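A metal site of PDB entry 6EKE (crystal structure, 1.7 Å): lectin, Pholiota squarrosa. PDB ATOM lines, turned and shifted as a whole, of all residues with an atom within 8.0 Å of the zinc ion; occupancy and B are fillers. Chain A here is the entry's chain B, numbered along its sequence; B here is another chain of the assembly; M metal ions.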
ATOM      1  N   CYS A  13     -12.297  28.650 -31.638  1.00  0.00           N
ATOM      2  CA  CYS A  13     -13.727  28.809 -31.836  1.00  0.00           C
ATOM      3  C   CYS A  13     -14.434  27.505 -31.576  1.00  0.00           C
ATOM      4  O   CYS A  13     -13.831  26.414 -31.566  1.00  0.00           O
ATOM      5  CB  CYS A  13     -14.046  29.327 -33.272  1.00  0.00           C
ATOM      6  SG  CYS A  13     -13.250  30.894 -33.730  1.00  0.00           S
ATOM      7  N   ASP A  14     -15.730  27.610 -31.379  1.00  0.00           N
ATOM      8  CA  ASP A  14     -16.432  26.464 -30.826  1.00  0.00           C
ATOM      9  C   ASP A  14     -17.742  26.297 -31.507  1.00  0.00           C
ATOM     10  O   ASP A  14     -18.633  27.120 -31.403  1.00  0.00           O
ATOM     11  CB  ASP A  14     -16.563  26.641 -29.337  1.00  0.00           C
ATOM     12  CG  ASP A  14     -16.970  25.370 -28.634  1.00  0.00           C
ATOM     13  OD1 ASP A  14     -17.213  24.370 -29.312  1.00  0.00           O
ATOM     14  OD2 ASP A  14     -17.051  25.396 -27.408  1.00  0.00           O
ATOM     15  N   GLY A  15     -17.880  25.168 -32.169  1.00  0.00           N
ATOM     16  CA  GLY A  15     -19.033  24.919 -32.966  1.00  0.00           C
ATOM     17  C   GLY A  15     -20.291  24.634 -32.159  1.00  0.00           C
ATOM     18  O   GLY A  15     -21.375  24.747 -32.716  1.00  0.00           O
ATOM     19  N   ASP A  16     -20.175  24.239 -30.880  1.00  0.00           N
ATOM     20  CA  ASP A  16     -21.377  23.944 -30.084  1.00  0.00           C
ATOM     21  C   ASP A  16     -21.898  25.109 -29.258  1.00  0.00           C
ATOM     22  O   ASP A  16     -23.072  25.119 -28.933  1.00  0.00           O
ATOM     23  CB  ASP A  16     -21.312  22.625 -29.302  1.00  0.00           C
ATOM     24  CG  ASP A  16     -20.368  22.625 -28.134  1.00  0.00           C
ATOM     25  OD1 ASP A  16     -19.371  23.395 -28.082  1.00  0.00           O
ATOM     26  OD2 ASP A  16     -20.574  21.742 -27.243  1.00  0.00           O
ATOM     27  N   THR A  17     -21.042  26.102 -29.010  1.00  0.00           N
ATOM     28  CA  THR A  17     -21.506  27.356 -28.412  1.00  0.00           C
ATOM     29  C   THR A  17     -21.576  28.500 -29.394  1.00  0.00           C
ATOM     30  O   THR A  17     -22.179  29.571 -29.063  1.00  0.00           O
ATOM     31  CB  THR A  17     -20.574  27.804 -27.290  1.00  0.00           C
ATOM     32  OG1 THR A  17     -19.234  27.962 -27.824  1.00  0.00           O
ATOM     33  CG2 THR A  17     -20.580  26.803 -26.206  1.00  0.00           C
ATOM     34  N   TYR A  18     -20.994  28.343 -30.578  1.00  0.00           N
ATOM     35  CA  TYR A  18     -20.992  29.391 -31.627  1.00  0.00           C
ATOM     36  C   TYR A  18     -20.301  30.638 -31.068  1.00  0.00           C
ATOM     37  O   TYR A  18     -20.834  31.728 -31.155  1.00  0.00           O
ATOM     38  CB  TYR A  18     -22.402  29.748 -32.080  1.00  0.00           C
ATOM     39  CG  TYR A  18     -23.035  28.632 -32.825  1.00  0.00           C
ATOM     40  CD1 TYR A  18     -22.738  28.430 -34.162  1.00  0.00           C
ATOM     41  CD2 TYR A  18     -23.889  27.724 -32.159  1.00  0.00           C
ATOM     42  CE1 TYR A  18     -23.292  27.368 -34.864  1.00  0.00           C
ATOM     43  CE2 TYR A  18     -24.443  26.662 -32.862  1.00  0.00           C
ATOM     44  CZ  TYR A  18     -24.136  26.504 -34.208  1.00  0.00           C
ATOM     45  OH  TYR A  18     -24.629  25.468 -34.916  1.00  0.00           O
ATOM     46  N   LYS A  19     -19.190  30.408 -30.361  1.00  0.00           N
ATOM     47  CA  LYS A  19     -18.392  31.479 -29.834  1.00  0.00           C
ATOM     48  C   LYS A  19     -16.955  31.257 -30.231  1.00  0.00           C
ATOM     49  O   LYS A  19     -16.477  30.112 -30.252  1.00  0.00           O
ATOM     50  CB  LYS A  19     -18.545  31.544 -28.313  1.00  0.00           C
ATOM     51  CG  LYS A  19     -19.856  32.181 -27.866  1.00  0.00           C
ATOM     52  CD  LYS A  19     -20.074  32.005 -26.390  1.00  0.00           C
ATOM     53  CE  LYS A  19     -21.378  32.615 -25.879  1.00  0.00           C
ATOM     54  NZ  LYS A  19     -21.723  34.013 -26.322  1.00  0.00           N
ATOM     55  N   GLY B   1     -22.048  15.565 -24.638  1.00  0.00           N
ATOM     56  CA  GLY B   1     -21.231  16.377 -23.708  1.00  0.00           C
ATOM     57  C   GLY B   1     -20.626  17.522 -24.460  1.00  0.00           C
ATOM     58  O   GLY B   1     -20.768  17.597 -25.692  1.00  0.00           O
ATOM     59  N   ALA B   2     -19.956  18.416 -23.748  1.00  0.00           N
ATOM     60  CA  ALA B   2     -19.413  19.643 -24.362  1.00  0.00           C
ATOM     61  C   ALA B   2     -18.271  19.347 -25.322  1.00  0.00           C
ATOM     62  O   ALA B   2     -17.373  18.589 -24.975  1.00  0.00           O
ATOM     63  CB  ALA B   2     -18.896  20.574 -23.270  1.00  0.00           C
ATOM     64  N   MET B   3     -18.261  19.974 -26.510  1.00  0.00           N
ATOM     65  CA  MET B   3     -17.124  19.844 -27.461  1.00  0.00           C
ATOM     66  C   MET B   3     -16.139  20.933 -27.112  1.00  0.00           C
ATOM     67  O   MET B   3     -16.543  22.091 -26.970  1.00  0.00           O
ATOM     68  CB  MET B   3     -17.571  19.993 -28.913  1.00  0.00           C
ATOM     69  CG  MET B   3     -18.743  19.114 -29.345  1.00  0.00           C
ATOM     70  SD  MET B   3     -19.321  19.367 -31.059  1.00  0.00           S
ATOM     71  CE  MET B   3     -17.810  19.158 -32.044  1.00  0.00           C
ATOM     72  N   ALA B   4     -14.869  20.594 -26.925  1.00  0.00           N
ATOM     73  CA  ALA B   4     -13.884  21.612 -26.624  1.00  0.00           C
ATOM     74  C   ALA B   4     -13.722  22.512 -27.881  1.00  0.00           C
ATOM     75  O   ALA B   4     -13.915  22.054 -29.010  1.00  0.00           O
ATOM     76  CB  ALA B   4     -12.557  20.955 -26.284  1.00  0.00           C
ATOM     77  N   PRO B   5     -13.449  23.800 -27.674  1.00  0.00           N
ATOM     78  CA  PRO B   5     -13.112  24.666 -28.808  1.00  0.00           C
ATOM     79  C   PRO B   5     -11.909  24.161 -29.577  1.00  0.00           C
ATOM     80  O   PRO B   5     -11.002  23.549 -29.007  1.00  0.00           O
ATOM     81  CB  PRO B   5     -12.741  26.005 -28.149  1.00  0.00           C
ATOM     82  CG  PRO B   5     -13.460  26.000 -26.851  1.00  0.00           C
ATOM     83  CD  PRO B   5     -13.539  24.560 -26.424  1.00  0.00           C
ATOM     84  N   VAL B   6     -11.852  24.537 -30.854  1.00  0.00           N
ATOM     85  CA  VAL B   6     -10.735  24.112 -31.717  1.00  0.00           C
ATOM     86  C   VAL B   6      -9.889  25.335 -32.092  1.00  0.00           C
ATOM     87  O   VAL B   6     -10.432  26.446 -32.186  1.00  0.00           O
ATOM     88  CB  VAL B   6     -11.227  23.357 -32.979  1.00  0.00           C
ATOM     89  CG1 VAL B   6     -12.002  22.115 -32.559  1.00  0.00           C
ATOM     90  CG2 VAL B   6     -12.048  24.217 -33.931  1.00  0.00           C
HETATM   91 ZN    ZN M   1     -17.871  23.509 -27.039  1.00  0.00          ZN
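The zinc ion is bound by OD1 of Asp 16, 1.8 Å away. O of Met 3 of chain B is bound to the zinc ion (1.9 Å). OD2 of Asp 14 binds the zinc ion (2.1 Å). OD1 of Asp 14 binds the zinc ion, at 2.5 Å.
OG1 of Thr 17 sits close to OD2 of Asp 14, at 3.4 Å. N of Asp 14 is in hydrogen-bond range of O of Lys 19 (2.8 Å).
The nearest printed residue that does not touch the zinc ion is Ala 4 of chain B (4.2 Å).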
